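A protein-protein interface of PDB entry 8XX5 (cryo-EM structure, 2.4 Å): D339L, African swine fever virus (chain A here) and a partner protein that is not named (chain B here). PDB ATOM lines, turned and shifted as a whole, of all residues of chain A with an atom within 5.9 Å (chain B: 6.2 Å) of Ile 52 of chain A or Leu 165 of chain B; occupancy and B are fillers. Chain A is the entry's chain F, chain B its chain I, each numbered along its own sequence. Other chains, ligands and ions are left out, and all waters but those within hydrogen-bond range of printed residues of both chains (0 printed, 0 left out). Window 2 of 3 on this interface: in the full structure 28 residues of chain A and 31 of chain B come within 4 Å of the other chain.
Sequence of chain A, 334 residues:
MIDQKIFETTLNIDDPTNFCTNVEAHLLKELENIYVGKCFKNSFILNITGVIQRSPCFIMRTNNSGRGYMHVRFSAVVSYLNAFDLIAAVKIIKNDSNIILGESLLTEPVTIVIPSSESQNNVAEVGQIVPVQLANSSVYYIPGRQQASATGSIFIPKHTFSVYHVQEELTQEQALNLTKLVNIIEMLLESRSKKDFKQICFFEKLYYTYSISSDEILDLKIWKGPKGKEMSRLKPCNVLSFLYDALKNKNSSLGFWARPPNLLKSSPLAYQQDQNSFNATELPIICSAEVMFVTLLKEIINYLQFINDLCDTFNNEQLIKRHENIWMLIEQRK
The side-chain amide nitrogen (NE2) of Gln 53 of chain A sits at hydrogen-bond distance from the backbone carbonyl oxygen (O) of Leu 165 of chain B (3.4 Å). The guanidinium group (NH2) of Arg 73 of chain A lies within salt-bridge range of the side-chain carboxylate (OE2) of Glu 168 of chain B. The side-chain carboxylate of Glu 168 of chain B lies within hydrogen-bond range of the side-chain amide nitrogen of Gln 53 of chain A (3.3 Å).
O of Gln 53 of chain A lies within hydrogen-bond range of N of Arg 73 of chain A, 2.7 Å away. The backbone carbonyl oxygen (O) of Arg 73 of chain A sits at hydrogen-bond distance from the backbone NH (N) of Ile 52 of chain A, 2.8 Å away.
Among the printed residues, merely in contact across the chains: Arg 73 of chain A with Leu 165 of chain B, Ile 6 of chain A with His 162 of chain B, Ile 52 of chain A with Leu 165 of chain B and Ile 6 of chain A with Val 161 of chain B.
Ile 52 of chain A touches just one residue of chain B: Leu 165 (3.6 Å). Of the printed residues of chain A, Glu 168 of chain B touches Gln 53 (3.3 Å) and Arg 73 (3.6 Å). Of the printed residues of chain B, Ile 6 of chain A touches Val 161 (3.7 Å) and His 162 (3.6 Å). Printed residues of chain B within 4 Å of Gln 53 of chain A: Leu 165 (3.4 Å) and Glu 168 (3.3 Å). Of the printed residues of chain B, Arg 73 of chain A touches Leu 165 and Glu 168. Of the printed residues of chain A, Val 161 of chain B touches Ile 6 (3.7 Å). The nearest residue of chain B that does not touch Ile 52 of chain A is His 162 of chain B (4.8 Å).
Of the 10 printed residues of chain B, 4 touch a printed residue of chain A. Printed residues of chain B that touch a printed residue of chain A: Val 161, His 162, Leu 165 and Glu 168. Hydrophobic or aromatic side chains of chain B that line the printed part of chain A: Val 161, His 162 and Leu 165. Hydrophobic or aromatic side chains of chain A that line the printed part of chain B: Ile 6 and Ile 52.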
ATOM      1  N   ILE A   6      28.929 -13.612  -3.203  1.00  0.00           N
ATOM      2  CA  ILE A   6      28.448 -14.927  -3.610  1.00  0.00           C
ATOM      3  C   ILE A   6      28.115 -14.875  -5.094  1.00  0.00           C
ATOM      4  O   ILE A   6      27.336 -14.020  -5.532  1.00  0.00           O
ATOM      5  CB  ILE A   6      27.226 -15.359  -2.783  1.00  0.00           C
ATOM      6  CG1 ILE A   6      27.616 -15.522  -1.314  1.00  0.00           C
ATOM      7  CG2 ILE A   6      26.641 -16.650  -3.328  1.00  0.00           C
ATOM      8  CD1 ILE A   6      26.447 -15.768  -0.393  1.00  0.00           C
ATOM      9  N   PHE A   7      28.703 -15.786  -5.865  1.00  0.00           N
ATOM     10  CA  PHE A   7      28.514 -15.840  -7.305  1.00  0.00           C
ATOM     11  C   PHE A   7      27.868 -17.158  -7.708  1.00  0.00           C
ATOM     12  O   PHE A   7      28.028 -18.180  -7.037  1.00  0.00           O
ATOM     13  CB  PHE A   7      29.840 -15.686  -8.053  1.00  0.00           C
ATOM     14  CG  PHE A   7      30.521 -14.377  -7.814  1.00  0.00           C
ATOM     15  CD1 PHE A   7      31.385 -14.217  -6.748  1.00  0.00           C
ATOM     16  CD2 PHE A   7      30.299 -13.305  -8.658  1.00  0.00           C
ATOM     17  CE1 PHE A   7      32.012 -13.015  -6.528  1.00  0.00           C
ATOM     18  CE2 PHE A   7      30.924 -12.097  -8.441  1.00  0.00           C
ATOM     19  CZ  PHE A   7      31.780 -11.952  -7.374  1.00  0.00           C
ATOM     20  N   GLY A  50      35.221 -20.343  -0.942  1.00  0.00           N
ATOM     21  CA  GLY A  50      34.765 -21.716  -0.963  1.00  0.00           C
ATOM     22  C   GLY A  50      33.475 -21.833  -1.743  1.00  0.00           C
ATOM     23  O   GLY A  50      32.915 -20.845  -2.223  1.00  0.00           O
ATOM     24  N   VAL A  51      33.014 -23.074  -1.858  1.00  0.00           N
ATOM     25  CA  VAL A  51      31.786 -23.398  -2.575  1.00  0.00           C
ATOM     26  C   VAL A  51      30.670 -23.564  -1.555  1.00  0.00           C
ATOM     27  O   VAL A  51      30.772 -24.389  -0.639  1.00  0.00           O
ATOM     28  CB  VAL A  51      31.953 -24.668  -3.422  1.00  0.00           C
ATOM     29  CG1 VAL A  51      30.676 -24.968  -4.187  1.00  0.00           C
ATOM     30  CG2 VAL A  51      33.128 -24.517  -4.373  1.00  0.00           C
ATOM     31  N   ILE A  52      29.604 -22.781  -1.707  1.00  0.00           N
ATOM     32  CA  ILE A  52      28.447 -22.921  -0.830  1.00  0.00           C
ATOM     33  C   ILE A  52      27.568 -24.074  -1.290  1.00  0.00           C
ATOM     34  O   ILE A  52      27.320 -25.030  -0.546  1.00  0.00           O
ATOM     35  CB  ILE A  52      27.646 -21.609  -0.770  1.00  0.00           C
ATOM     36  CG1 ILE A  52      28.549 -20.439  -0.394  1.00  0.00           C
ATOM     37  CG2 ILE A  52      26.496 -21.738   0.212  1.00  0.00           C
ATOM     38  CD1 ILE A  52      28.289 -19.204  -1.213  1.00  0.00           C
ATOM     39  N   GLN A  53      27.084 -23.996  -2.525  1.00  0.00           N
ATOM     40  CA  GLN A  53      26.231 -25.020  -3.099  1.00  0.00           C
ATOM     41  C   GLN A  53      26.724 -25.341  -4.498  1.00  0.00           C
ATOM     42  O   GLN A  53      27.368 -24.520  -5.152  1.00  0.00           O
ATOM     43  CB  GLN A  53      24.762 -24.582  -3.148  1.00  0.00           C
ATOM     44  CG  GLN A  53      24.078 -24.567  -1.798  1.00  0.00           C
ATOM     45  CD  GLN A  53      22.600 -24.268  -1.900  1.00  0.00           C
ATOM     46  OE1 GLN A  53      22.069 -24.070  -2.992  1.00  0.00           O
ATOM     47  NE2 GLN A  53      21.924 -24.234  -0.760  1.00  0.00           N
ATOM     48  N   ARG A  54      26.416 -26.552  -4.948  1.00  0.00           N
ATOM     49  CA  ARG A  54      26.851 -27.008  -6.255  1.00  0.00           C
ATOM     50  C   ARG A  54      25.837 -28.005  -6.790  1.00  0.00           C
ATOM     51  O   ARG A  54      25.022 -28.552  -6.046  1.00  0.00           O
ATOM     52  CB  ARG A  54      28.248 -27.631  -6.194  1.00  0.00           C
ATOM     53  CG  ARG A  54      28.227 -29.101  -5.856  1.00  0.00           C
ATOM     54  CD  ARG A  54      29.508 -29.794  -6.254  1.00  0.00           C
ATOM     55  NE  ARG A  54      29.726 -30.978  -5.436  1.00  0.00           N
ATOM     56  CZ  ARG A  54      29.621 -32.221  -5.884  1.00  0.00           C
ATOM     57  NH1 ARG A  54      29.294 -32.476  -7.139  1.00  0.00           N
ATOM     58  NH2 ARG A  54      29.850 -33.231  -5.052  1.00  0.00           N
ATOM     59  N   ARG A  73      27.837 -22.526  -6.916  1.00  0.00           N
ATOM     60  CA  ARG A  73      27.457 -21.334  -6.162  1.00  0.00           C
ATOM     61  C   ARG A  73      28.522 -21.129  -5.089  1.00  0.00           C
ATOM     62  O   ARG A  73      28.494 -21.786  -4.045  1.00  0.00           O
ATOM     63  CB  ARG A  73      26.066 -21.486  -5.557  1.00  0.00           C
ATOM     64  CG  ARG A  73      25.615 -20.309  -4.721  1.00  0.00           C
ATOM     65  CD  ARG A  73      24.178 -19.941  -5.033  1.00  0.00           C
ATOM     66  NE  ARG A  73      23.250 -21.010  -4.684  1.00  0.00           N
ATOM     67  CZ  ARG A  73      21.975 -21.042  -5.046  1.00  0.00           C
ATOM     68  NH1 ARG A  73      21.442 -20.082  -5.782  1.00  0.00           N
ATOM     69  NH2 ARG A  73      21.217 -22.062  -4.659  1.00  0.00           N
ATOM     70  N   PHE A  74      29.460 -20.224  -5.345  1.00  0.00           N
ATOM     71  CA  PHE A  74      30.640 -20.069  -4.511  1.00  0.00           C
ATOM     72  C   PHE A  74      30.724 -18.661  -3.939  1.00  0.00           C
ATOM     73  O   PHE A  74      30.288 -17.688  -4.562  1.00  0.00           O
ATOM     74  CB  PHE A  74      31.918 -20.378  -5.298  1.00  0.00           C
ATOM     75  CG  PHE A  74      32.172 -19.437  -6.444  1.00  0.00           C
ATOM     76  CD1 PHE A  74      31.517 -19.601  -7.652  1.00  0.00           C
ATOM     77  CD2 PHE A  74      33.075 -18.396  -6.314  1.00  0.00           C
ATOM     78  CE1 PHE A  74      31.753 -18.741  -8.704  1.00  0.00           C
ATOM     79  CE2 PHE A  74      33.315 -17.534  -7.363  1.00  0.00           C
ATOM     80  CZ  PHE A  74      32.653 -17.707  -8.560  1.00  0.00           C
ATOM     81  N   SER A  75      31.296 -18.569  -2.744  1.00  0.00           N
ATOM     82  CA  SER A  75      31.571 -17.298  -2.091  1.00  0.00           C
ATOM     83  C   SER A  75      33.011 -16.899  -2.381  1.00  0.00           C
ATOM     84  O   SER A  75      33.923 -17.723  -2.260  1.00  0.00           O
ATOM     85  CB  SER A  75      31.340 -17.397  -0.583  1.00  0.00           C
ATOM     86  OG  SER A  75      31.256 -16.115   0.008  1.00  0.00           O
ATOM     87  N   MET B 160      21.341 -11.681   2.984  1.00  0.00           N
ATOM     88  CA  MET B 160      20.103 -12.329   2.560  1.00  0.00           C
ATOM     89  C   MET B 160      20.377 -13.598   1.758  1.00  0.00           C
ATOM     90  O   MET B 160      19.742 -14.635   1.992  1.00  0.00           O
ATOM     91  CB  MET B 160      19.248 -11.356   1.749  1.00  0.00           C
ATOM     92  CG  MET B 160      18.826 -10.108   2.511  1.00  0.00           C
ATOM     93  SD  MET B 160      17.166  -9.545   2.091  1.00  0.00           S
ATOM     94  CE  MET B 160      16.204 -11.009   2.459  1.00  0.00           C
ATOM     95  N   VAL B 161      21.316 -13.543   0.806  1.00  0.00           N
ATOM     96  CA  VAL B 161      21.624 -14.731   0.013  1.00  0.00           C
ATOM     97  C   VAL B 161      22.207 -15.826   0.896  1.00  0.00           C
ATOM     98  O   VAL B 161      21.852 -17.003   0.763  1.00  0.00           O
ATOM     99  CB  VAL B 161      22.568 -14.375  -1.152  1.00  0.00           C
ATOM    100  CG1 VAL B 161      23.070 -15.635  -1.835  1.00  0.00           C
ATOM    101  CG2 VAL B 161      21.858 -13.492  -2.153  1.00  0.00           C
ATOM    102  N   HIS B 162      23.104 -15.459   1.815  1.00  0.00           N
ATOM    103  CA  HIS B 162      23.701 -16.438   2.715  1.00  0.00           C
ATOM    104  C   HIS B 162      22.652 -17.074   3.615  1.00  0.00           C
ATOM    105  O   HIS B 162      22.684 -18.284   3.856  1.00  0.00           O
ATOM    106  CB  HIS B 162      24.794 -15.770   3.549  1.00  0.00           C
ATOM    107  CG  HIS B 162      25.938 -16.674   3.887  1.00  0.00           C
ATOM    108  ND1 HIS B 162      26.933 -16.984   2.985  1.00  0.00           N
ATOM    109  CD2 HIS B 162      26.253 -17.323   5.032  1.00  0.00           C
ATOM    110  CE1 HIS B 162      27.807 -17.792   3.558  1.00  0.00           C
ATOM    111  NE2 HIS B 162      27.418 -18.014   4.800  1.00  0.00           N
ATOM    112  N   ARG B 163      21.718 -16.271   4.129  1.00  0.00           N
ATOM    113  CA  ARG B 163      20.651 -16.809   4.963  1.00  0.00           C
ATOM    114  C   ARG B 163      19.760 -17.758   4.175  1.00  0.00           C
ATOM    115  O   ARG B 163      19.378 -18.822   4.676  1.00  0.00           O
ATOM    116  CB  ARG B 163      19.833 -15.663   5.555  1.00  0.00           C
ATOM    117  CG  ARG B 163      18.992 -16.048   6.752  1.00  0.00           C
ATOM    118  CD  ARG B 163      17.518 -15.791   6.488  1.00  0.00           C
ATOM    119  NE  ARG B 163      16.935 -16.785   5.594  1.00  0.00           N
ATOM    120  CZ  ARG B 163      16.198 -16.496   4.530  1.00  0.00           C
ATOM    121  NH1 ARG B 163      15.941 -15.246   4.185  1.00  0.00           N
ATOM    122  NH2 ARG B 163      15.704 -17.489   3.796  1.00  0.00           N
ATOM    123  N   LYS B 164      19.419 -17.392   2.938  1.00  0.00           N
ATOM    124  CA  LYS B 164      18.604 -18.273   2.107  1.00  0.00           C
ATOM    125  C   LYS B 164      19.322 -19.588   1.829  1.00  0.00           C
ATOM    126  O   LYS B 164      18.721 -20.665   1.906  1.00  0.00           O
ATOM    127  CB  LYS B 164      18.243 -17.573   0.799  1.00  0.00           C
ATOM    128  CG  LYS B 164      17.113 -18.233   0.029  1.00  0.00           C
ATOM    129  CD  LYS B 164      17.101 -17.788  -1.426  1.00  0.00           C
ATOM    130  CE  LYS B 164      18.487 -17.868  -2.046  1.00  0.00           C
ATOM    131  NZ  LYS B 164      18.463 -18.524  -3.384  1.00  0.00           N
ATOM    132  N   LEU B 165      20.614 -19.519   1.503  1.00  0.00           N
ATOM    133  CA  LEU B 165      21.363 -20.730   1.183  1.00  0.00           C
ATOM    134  C   LEU B 165      21.527 -21.619   2.410  1.00  0.00           C
ATOM    135  O   LEU B 165      21.365 -22.842   2.330  1.00  0.00           O
ATOM    136  CB  LEU B 165      22.722 -20.363   0.587  1.00  0.00           C
ATOM    137  CG  LEU B 165      22.669 -19.631  -0.755  1.00  0.00           C
ATOM    138  CD1 LEU B 165      24.038 -19.580  -1.407  1.00  0.00           C
ATOM    139  CD2 LEU B 165      21.652 -20.281  -1.677  1.00  0.00           C
ATOM    140  N   ASP B 166      21.844 -21.021   3.559  1.00  0.00           N
ATOM    141  CA  ASP B 166      21.994 -21.794   4.784  1.00  0.00           C
ATOM    142  C   ASP B 166      20.663 -22.314   5.309  1.00  0.00           C
ATOM    143  O   ASP B 166      20.656 -23.272   6.088  1.00  0.00           O
ATOM    144  CB  ASP B 166      22.684 -20.944   5.853  1.00  0.00           C
ATOM    145  CG  ASP B 166      24.181 -21.173   5.902  1.00  0.00           C
ATOM    146  OD1 ASP B 166      24.635 -22.249   5.455  1.00  0.00           O
ATOM    147  OD2 ASP B 166      24.906 -20.278   6.384  1.00  0.00           O
ATOM    148  N   ARG B 167      19.547 -21.708   4.908  1.00  0.00           N
ATOM    149  CA  ARG B 167      18.227 -22.213   5.262  1.00  0.00           C
ATOM    150  C   ARG B 167      17.810 -23.379   4.372  1.00  0.00           C
ATOM    151  O   ARG B 167      16.962 -24.187   4.760  1.00  0.00           O
ATOM    152  CB  ARG B 167      17.194 -21.085   5.178  1.00  0.00           C
ATOM    153  CG  ARG B 167      16.812 -20.495   6.525  1.00  0.00           C
ATOM    154  CD  ARG B 167      15.549 -19.646   6.420  1.00  0.00           C
ATOM    155  NE  ARG B 167      14.516 -20.252   5.584  1.00  0.00           N
ATOM    156  CZ  ARG B 167      13.909 -21.405   5.837  1.00  0.00           C
ATOM    157  NH1 ARG B 167      14.166 -22.102   6.932  1.00  0.00           N
ATOM    158  NH2 ARG B 167      13.011 -21.868   4.971  1.00  0.00           N
ATOM    159  N   GLU B 168      18.393 -23.470   3.176  1.00  0.00           N
ATOM    160  CA  GLU B 168      18.111 -24.569   2.260  1.00  0.00           C
ATOM    161  C   GLU B 168      18.518 -25.900   2.878  1.00  0.00           C
ATOM    162  O   GLU B 168      17.772 -26.881   2.802  1.00  0.00           O
ATOM    163  CB  GLU B 168      18.837 -24.358   0.929  1.00  0.00           C
ATOM    164  CG  GLU B 168      18.266 -23.239   0.074  1.00  0.00           C
ATOM    165  CD  GLU B 168      18.663 -23.360  -1.384  1.00  0.00           C
ATOM    166  OE1 GLU B 168      18.827 -24.500  -1.866  1.00  0.00           O
ATOM    167  OE2 GLU B 168      18.813 -22.313  -2.049  1.00  0.00           O
ATOM    168  N   ASP B 169      19.696 -25.938   3.493  1.00  0.00           N
ATOM    169  CA  ASP B 169      20.201 -27.152   4.120  1.00  0.00           C
ATOM    170  C   ASP B 169      21.315 -26.813   5.105  1.00  0.00           C
ATOM    171  O   ASP B 169      21.885 -25.722   5.060  1.00  0.00           O
ATOM    172  CB  ASP B 169      20.706 -28.136   3.059  1.00  0.00           C
ATOM    173  CG  ASP B 169      20.843 -29.554   3.588  1.00  0.00           C
ATOM    174  OD1 ASP B 169      21.031 -29.729   4.810  1.00  0.00           O
ATOM    175  OD2 ASP B 169      20.761 -30.500   2.775  1.00  0.00           O
